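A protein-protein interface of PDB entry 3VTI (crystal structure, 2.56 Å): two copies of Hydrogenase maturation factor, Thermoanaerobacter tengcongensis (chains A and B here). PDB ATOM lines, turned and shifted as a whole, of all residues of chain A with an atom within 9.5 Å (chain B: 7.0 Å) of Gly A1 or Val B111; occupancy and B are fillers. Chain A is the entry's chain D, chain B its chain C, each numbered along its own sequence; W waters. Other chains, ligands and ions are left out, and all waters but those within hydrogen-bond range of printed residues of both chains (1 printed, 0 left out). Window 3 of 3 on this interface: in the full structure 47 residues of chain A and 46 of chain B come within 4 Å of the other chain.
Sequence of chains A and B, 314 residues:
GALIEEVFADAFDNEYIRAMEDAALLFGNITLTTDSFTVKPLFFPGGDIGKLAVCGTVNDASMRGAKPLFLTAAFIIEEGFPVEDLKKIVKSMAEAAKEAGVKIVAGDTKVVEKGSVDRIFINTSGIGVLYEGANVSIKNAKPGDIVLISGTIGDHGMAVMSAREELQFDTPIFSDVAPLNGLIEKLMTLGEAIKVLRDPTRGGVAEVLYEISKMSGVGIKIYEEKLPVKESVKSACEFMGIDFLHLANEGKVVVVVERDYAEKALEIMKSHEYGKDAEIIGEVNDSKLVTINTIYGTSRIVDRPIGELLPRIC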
ATOM      1  N   GLY A   1      33.786 -23.133  15.405  1.00  0.00           N
ATOM      2  CA  GLY A   1      32.688 -23.868  14.707  1.00  0.00           C
ATOM      3  C   GLY A   1      31.307 -23.532  15.246  1.00  0.00           C
ATOM      4  O   GLY A   1      30.644 -22.622  14.746  1.00  0.00           O
ATOM      5  N   ALA A   2      30.885 -24.272  16.277  1.00  0.00           N
ATOM      6  CA  ALA A   2      29.558 -24.109  16.900  1.00  0.00           C
ATOM      7  C   ALA A   2      29.546 -23.095  18.065  1.00  0.00           C
ATOM      8  O   ALA A   2      28.662 -23.120  18.930  1.00  0.00           O
ATOM      9  CB  ALA A   2      29.013 -25.475  17.349  1.00  0.00           C
ATOM     10  N   LEU A   3      30.538 -22.205  18.066  1.00  0.00           N
ATOM     11  CA  LEU A   3      30.622 -21.083  19.004  1.00  0.00           C
ATOM     12  C   LEU A   3      29.686 -19.954  18.543  1.00  0.00           C
ATOM     13  O   LEU A   3      29.391 -19.019  19.294  1.00  0.00           O
ATOM     14  CB  LEU A   3      32.080 -20.598  19.066  1.00  0.00           C
ATOM     15  CG  LEU A   3      32.625 -19.821  20.268  1.00  0.00           C
ATOM     16  CD1 LEU A   3      33.998 -20.349  20.655  1.00  0.00           C
ATOM     17  CD2 LEU A   3      32.683 -18.328  19.987  1.00  0.00           C
ATOM     18  N   ILE A   4      29.213 -20.072  17.303  1.00  0.00           N
ATOM     19  CA  ILE A   4      28.395 -19.053  16.645  1.00  0.00           C
ATOM     20  C   ILE A   4      26.919 -19.183  17.030  1.00  0.00           C
ATOM     21  O   ILE A   4      26.274 -18.193  17.379  1.00  0.00           O
ATOM     22  CB  ILE A   4      28.557 -19.125  15.094  1.00  0.00           C
ATOM     23  CG1 ILE A   4      30.042 -19.124  14.678  1.00  0.00           C
ATOM     24  CG2 ILE A   4      27.776 -18.019  14.404  1.00  0.00           C
ATOM     25  CD1 ILE A   4      30.899 -17.960  15.212  1.00  0.00           C
ATOM     26  N   GLU A   5      26.397 -20.408  16.963  1.00  0.00           N
ATOM     27  CA  GLU A   5      25.031 -20.716  17.396  1.00  0.00           C
ATOM     28  C   GLU A   5      24.824 -20.423  18.885  1.00  0.00           C
ATOM     29  O   GLU A   5      23.691 -20.341  19.360  1.00  0.00           O
ATOM     30  CB  GLU A   5      24.693 -22.181  17.095  1.00  0.00           C
ATOM     31  CG  GLU A   5      25.614 -23.194  17.781  1.00  0.00           C
ATOM     32  CD  GLU A   5      25.294 -24.639  17.426  1.00  0.00           C
ATOM     33  OE1 GLU A   5      24.633 -24.876  16.390  1.00  0.00           O
ATOM     34  OE2 GLU A   5      25.713 -25.544  18.184  1.00  0.00           O
ATOM     35  N   GLU A   6      25.934 -20.282  19.607  1.00  0.00           N
ATOM     36  CA  GLU A   6      25.934 -19.869  21.004  1.00  0.00           C
ATOM     37  C   GLU A   6      25.561 -18.382  21.141  1.00  0.00           C
ATOM     38  O   GLU A   6      24.663 -18.034  21.918  1.00  0.00           O
ATOM     39  CB  GLU A   6      27.303 -20.170  21.641  1.00  0.00           C
ATOM     40  CG  GLU A   6      27.552 -19.547  23.019  1.00  0.00           C
ATOM     41  CD  GLU A   6      26.717 -20.176  24.124  1.00  0.00           C
ATOM     42  OE1 GLU A   6      25.472 -20.029  24.093  1.00  0.00           O
ATOM     43  OE2 GLU A   6      27.312 -20.805  25.030  1.00  0.00           O
ATOM     44  N   VAL A   7      26.249 -17.524  20.382  1.00  0.00           N
ATOM     45  CA  VAL A   7      25.953 -16.084  20.322  1.00  0.00           C
ATOM     46  C   VAL A   7      24.483 -15.863  19.940  1.00  0.00           C
ATOM     47  O   VAL A   7      23.800 -15.015  20.524  1.00  0.00           O
ATOM     48  CB  VAL A   7      26.872 -15.348  19.306  1.00  0.00           C
ATOM     49  CG1 VAL A   7      26.702 -13.835  19.410  1.00  0.00           C
ATOM     50  CG2 VAL A   7      28.329 -15.733  19.514  1.00  0.00           C
ATOM     51  N   SER A  36      19.255 -22.799   5.700  1.00  0.00           N
ATOM     52  CA  SER A  36      20.117 -22.442   4.576  1.00  0.00           C
ATOM     53  C   SER A  36      20.818 -23.674   4.053  1.00  0.00           C
ATOM     54  O   SER A  36      21.130 -24.584   4.817  1.00  0.00           O
ATOM     55  CB  SER A  36      21.167 -21.426   4.999  1.00  0.00           C
ATOM     56  OG  SER A  36      20.567 -20.203   5.340  1.00  0.00           O
ATOM     57  N   THR A  38      24.031 -24.957   1.670  1.00  0.00           N
ATOM     58  CA  THR A  38      25.342 -24.527   1.189  1.00  0.00           C
ATOM     59  C   THR A  38      26.162 -25.714   0.651  1.00  0.00           C
ATOM     60  O   THR A  38      27.379 -25.621   0.488  1.00  0.00           O
ATOM     61  CB  THR A  38      26.144 -23.835   2.328  1.00  0.00           C
ATOM     62  OG1 THR A  38      26.176 -24.691   3.476  1.00  0.00           O
ATOM     63  CG2 THR A  38      25.515 -22.486   2.725  1.00  0.00           C
ATOM     64  N   VAL A  39      25.469 -26.813   0.349  1.00  0.00           N
ATOM     65  CA  VAL A  39      26.094 -28.087  -0.030  1.00  0.00           C
ATOM     66  C   VAL A  39      26.898 -28.032  -1.329  1.00  0.00           C
ATOM     67  O   VAL A  39      26.488 -27.386  -2.293  1.00  0.00           O
ATOM     68  CB  VAL A  39      25.025 -29.212  -0.127  1.00  0.00           C
ATOM     69  CG1 VAL A  39      24.076 -28.998  -1.330  1.00  0.00           C
ATOM     70  CG2 VAL A  39      25.679 -30.571  -0.178  1.00  0.00           C
ATOM     71  N   PHE A 121      23.883 -20.058  -2.950  1.00  0.00           N
ATOM     72  CA  PHE A 121      23.338 -20.492  -1.671  1.00  0.00           C
ATOM     73  C   PHE A 121      21.841 -20.332  -1.721  1.00  0.00           C
ATOM     74  O   PHE A 121      21.337 -19.397  -2.330  1.00  0.00           O
ATOM     75  CB  PHE A 121      23.913 -19.683  -0.506  1.00  0.00           C
ATOM     76  CG  PHE A 121      25.362 -19.991  -0.205  1.00  0.00           C
ATOM     77  CD1 PHE A 121      25.905 -21.242  -0.500  1.00  0.00           C
ATOM     78  CD2 PHE A 121      26.183 -19.030   0.381  1.00  0.00           C
ATOM     79  CE1 PHE A 121      27.249 -21.528  -0.233  1.00  0.00           C
ATOM     80  CE2 PHE A 121      27.539 -19.315   0.655  1.00  0.00           C
ATOM     81  CZ  PHE A 121      28.058 -20.571   0.355  1.00  0.00           C
ATOM     82  N   ARG A 202      22.483 -32.421   9.688  1.00  0.00           N
ATOM     83  CA  ARG A 202      23.869 -32.185  10.125  1.00  0.00           C
ATOM     84  C   ARG A 202      24.035 -32.564  11.599  1.00  0.00           C
ATOM     85  O   ARG A 202      23.271 -32.099  12.444  1.00  0.00           O
ATOM     86  CB  ARG A 202      24.286 -30.721   9.882  1.00  0.00           C
ATOM     87  CG  ARG A 202      25.797 -30.468   9.984  1.00  0.00           C
ATOM     88  CD  ARG A 202      26.154 -28.974   9.836  1.00  0.00           C
ATOM     89  NE  ARG A 202      27.452 -28.670  10.454  1.00  0.00           N
ATOM     90  CZ  ARG A 202      27.619 -28.221  11.705  1.00  0.00           C
ATOM     91  NH1 ARG A 202      26.567 -28.005  12.501  1.00  0.00           N
ATOM     92  NH2 ARG A 202      28.844 -27.978  12.162  1.00  0.00           N
ATOM     93  N   PHE B  75      21.974 -17.131   9.159  1.00  0.00           N
ATOM     94  CA  PHE B  75      23.303 -16.564   9.036  1.00  0.00           C
ATOM     95  C   PHE B  75      24.201 -17.516   8.264  1.00  0.00           C
ATOM     96  O   PHE B  75      24.291 -18.702   8.593  1.00  0.00           O
ATOM     97  CB  PHE B  75      23.922 -16.356  10.415  1.00  0.00           C
ATOM     98  CG  PHE B  75      23.148 -15.439  11.310  1.00  0.00           C
ATOM     99  CD1 PHE B  75      22.162 -15.943  12.163  1.00  0.00           C
ATOM    100  CD2 PHE B  75      23.428 -14.081  11.334  1.00  0.00           C
ATOM    101  CE1 PHE B  75      21.453 -15.108  13.007  1.00  0.00           C
ATOM    102  CE2 PHE B  75      22.725 -13.232  12.171  1.00  0.00           C
ATOM    103  CZ  PHE B  75      21.730 -13.751  13.017  1.00  0.00           C
ATOM    104  N   ILE B  76      24.872 -16.993   7.243  1.00  0.00           N
ATOM    105  CA  ILE B  76      25.857 -17.761   6.502  1.00  0.00           C
ATOM    106  C   ILE B  76      27.209 -17.069   6.695  1.00  0.00           C
ATOM    107  O   ILE B  76      27.410 -15.966   6.181  1.00  0.00           O
ATOM    108  CB  ILE B  76      25.470 -17.889   5.002  1.00  0.00           C
ATOM    109  CG1 ILE B  76      24.098 -18.578   4.871  1.00  0.00           C
ATOM    110  CG2 ILE B  76      26.549 -18.631   4.233  1.00  0.00           C
ATOM    111  CD1 ILE B  76      23.447 -18.494   3.503  1.00  0.00           C
ATOM    112  N   ILE B  77      28.112 -17.704   7.451  1.00  0.00           N
ATOM    113  CA  ILE B  77      29.329 -17.044   7.928  1.00  0.00           C
ATOM    114  C   ILE B  77      30.615 -17.679   7.411  1.00  0.00           C
ATOM    115  O   ILE B  77      30.766 -18.902   7.411  1.00  0.00           O
ATOM    116  CB  ILE B  77      29.390 -16.999   9.478  1.00  0.00           C
ATOM    117  CG1 ILE B  77      28.150 -16.316  10.060  1.00  0.00           C
ATOM    118  CG2 ILE B  77      30.633 -16.280   9.963  1.00  0.00           C
ATOM    119  CD1 ILE B  77      27.251 -17.265  10.807  1.00  0.00           C
ATOM    120  N   GLU B  78      31.541 -16.822   6.984  1.00  0.00           N
ATOM    121  CA  GLU B  78      32.871 -17.236   6.537  1.00  0.00           C
ATOM    122  C   GLU B  78      33.725 -17.733   7.708  1.00  0.00           C
ATOM    123  O   GLU B  78      33.749 -17.130   8.777  1.00  0.00           O
ATOM    124  CB  GLU B  78      33.570 -16.074   5.824  1.00  0.00           C
ATOM    125  CG  GLU B  78      34.794 -16.461   4.984  1.00  0.00           C
ATOM    126  CD  GLU B  78      35.408 -15.278   4.237  1.00  0.00           C
ATOM    127  OE1 GLU B  78      35.327 -14.135   4.741  1.00  0.00           O
ATOM    128  OE2 GLU B  78      35.970 -15.491   3.142  1.00  0.00           O
ATOM    129  N   GLU B  79      34.412 -18.850   7.491  1.00  0.00           N
ATOM    130  CA  GLU B  79      35.433 -19.348   8.411  1.00  0.00           C
ATOM    131  C   GLU B  79      36.354 -18.196   8.841  1.00  0.00           C
ATOM    132  O   GLU B  79      36.916 -17.485   7.998  1.00  0.00           O
ATOM    133  CB  GLU B  79      36.236 -20.451   7.715  1.00  0.00           C
ATOM    134  CG  GLU B  79      37.291 -21.168   8.568  1.00  0.00           C
ATOM    135  CD  GLU B  79      36.770 -22.447   9.208  1.00  0.00           C
ATOM    136  OE1 GLU B  79      35.598 -22.816   8.966  1.00  0.00           O
ATOM    137  OE2 GLU B  79      37.534 -23.085   9.959  1.00  0.00           O
ATOM    138  N   GLY B  80      36.465 -17.991  10.149  1.00  0.00           N
ATOM    139  CA  GLY B  80      37.385 -16.992  10.690  1.00  0.00           C
ATOM    140  C   GLY B  80      36.921 -15.547  10.651  1.00  0.00           C
ATOM    141  O   GLY B  80      37.737 -14.634  10.831  1.00  0.00           O
ATOM    142  N   THR B 109      22.373 -21.202  11.605  1.00  0.00           N
ATOM    143  CA  THR B 109      23.715 -20.691  11.386  1.00  0.00           C
ATOM    144  C   THR B 109      24.543 -21.737  10.640  1.00  0.00           C
ATOM    145  O   THR B 109      24.607 -22.899  11.040  1.00  0.00           O
ATOM    146  CB  THR B 109      24.417 -20.311  12.704  1.00  0.00           C
ATOM    147  OG1 THR B 109      24.269 -21.374  13.652  1.00  0.00           O
ATOM    148  CG2 THR B 109      23.821 -19.049  13.298  1.00  0.00           C
ATOM    149  N   LYS B 110      25.149 -21.315   9.534  1.00  0.00           N
ATOM    150  CA  LYS B 110      26.028 -22.164   8.748  1.00  0.00           C
ATOM    151  C   LYS B 110      27.363 -21.468   8.633  1.00  0.00           C
ATOM    152  O   LYS B 110      27.422 -20.258   8.385  1.00  0.00           O
ATOM    153  CB  LYS B 110      25.470 -22.406   7.341  1.00  0.00           C
ATOM    154  CG  LYS B 110      24.249 -23.310   7.266  1.00  0.00           C
ATOM    155  CD  LYS B 110      24.596 -24.774   7.518  1.00  0.00           C
ATOM    156  CE  LYS B 110      23.429 -25.709   7.178  1.00  0.00           C
ATOM    157  NZ  LYS B 110      22.224 -25.505   8.044  1.00  0.00           N
ATOM    158  N   VAL B 111      28.425 -22.245   8.819  1.00  0.00           N
ATOM    159  CA  VAL B 111      29.788 -21.776   8.649  1.00  0.00           C
ATOM    160  C   VAL B 111      30.363 -22.436   7.397  1.00  0.00           C
ATOM    161  O   VAL B 111      30.347 -23.658   7.273  1.00  0.00           O
ATOM    162  CB  VAL B 111      30.654 -22.117   9.885  1.00  0.00           C
ATOM    163  CG1 VAL B 111      32.075 -21.603   9.719  1.00  0.00           C
ATOM    164  CG2 VAL B 111      30.028 -21.546  11.154  1.00  0.00           C
ATOM    165  N   VAL B 112      30.864 -21.628   6.469  1.00  0.00           N
ATOM    166  CA  VAL B 112      31.447 -22.134   5.217  1.00  0.00           C
ATOM    167  C   VAL B 112      32.947 -21.859   5.154  1.00  0.00           C
ATOM    168  O   VAL B 112      33.427 -20.963   5.848  1.00  0.00           O
ATOM    169  CB  VAL B 112      30.736 -21.525   3.985  1.00  0.00           C
ATOM    170  CG1 VAL B 112      29.334 -22.102   3.849  1.00  0.00           C
ATOM    171  CG2 VAL B 112      30.668 -20.005   4.099  1.00  0.00           C
ATOM    172  N   GLU B 113      33.672 -22.625   4.328  1.00  0.00           N
ATOM    173  CA  GLU B 113      35.136 -22.481   4.152  1.00  0.00           C
ATOM    174  C   GLU B 113      35.527 -21.038   3.886  1.00  0.00           C
ATOM    175  O   GLU B 113      34.749 -20.272   3.314  1.00  0.00           O
ATOM    176  CB  GLU B 113      35.652 -23.300   2.964  1.00  0.00           C
ATOM    177  CG  GLU B 113      35.077 -24.689   2.803  1.00  0.00           C
ATOM    178  CD  GLU B 113      35.735 -25.702   3.706  1.00  0.00           C
ATOM    179  OE1 GLU B 113      36.977 -25.871   3.628  1.00  0.00           O
ATOM    180  OE2 GLU B 113      34.998 -26.338   4.490  1.00  0.00           O
HETATM  181  O   HOH W   1      21.707 -20.047   7.935  1.00  0.00           O
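O of Ile B77 sits at hydrogen-bond distance from N of Val B112 (2.9 Å). O of Phe B75 is in hydrogen-bond range of N of Lys B110, at 2.9 Å. The backbone NH (N) of Glu B79 sits at hydrogen-bond distance from the backbone carbonyl oxygen (O) of Val B112 (2.9 Å). The backbone carbonyl oxygen of Lys B110 is in hydrogen-bond range of the backbone NH of Ile B77, at 2.8 Å.
Gly A1 touches Val B111 (O to CG2, 3.8 Å). Ile B77 touches Ile A4. Thr B109 touches Glu A5 (OG1 to CB, 3.6 Å). Ser A36 touches Ile B76. Ser A36 touches Lys B110. Val B112 touches Thr A38 (CG1 to CB, 3.9 Å). CE2 of Phe A121 touches CG2 of Ile B76, 3.8 Å away.
Gly A1 touches just one residue of chain B: Val B111 (3.8 Å). Printed residues of chain B within 4 Å of Glu A5: Thr B109 (3.6 Å). Val A39 touches none of the printed residues of chain B. Printed residues of chain B within 4 Å of Phe A121: Ile B76. Of the printed residues of chain A, Ile B76 touches Ser A36 and Phe A121. Of the printed residues of chain A, Lys B110 touches Ser A36. Of chain A, only Gly A1 (3.8 Å) comes within 4 Å of Val B111. Of chain A, only Thr A38 comes within 4 Å of Val B112. The nearest residue of chain B that does not touch Gly A1 is Glu B79 (6.5 Å). The nearest residue of chain A that does not touch Val B111 is Ile A4 (4.3 Å). The nearest printed residue of chain A that does not touch Ile B76 is Thr A38 (4.3 Å).
Among the printed residues, 7 pairs touch across the chains.
No position is printed for both chains. Of the 7 pairs that touch across the chains among the printed residues, none has its exchanged pair printed and touching as well.
Water W1 lies within hydrogen-bond range of OG of Ser A36 (2.8 Å) and O of Phe B75 (3.0 Å).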
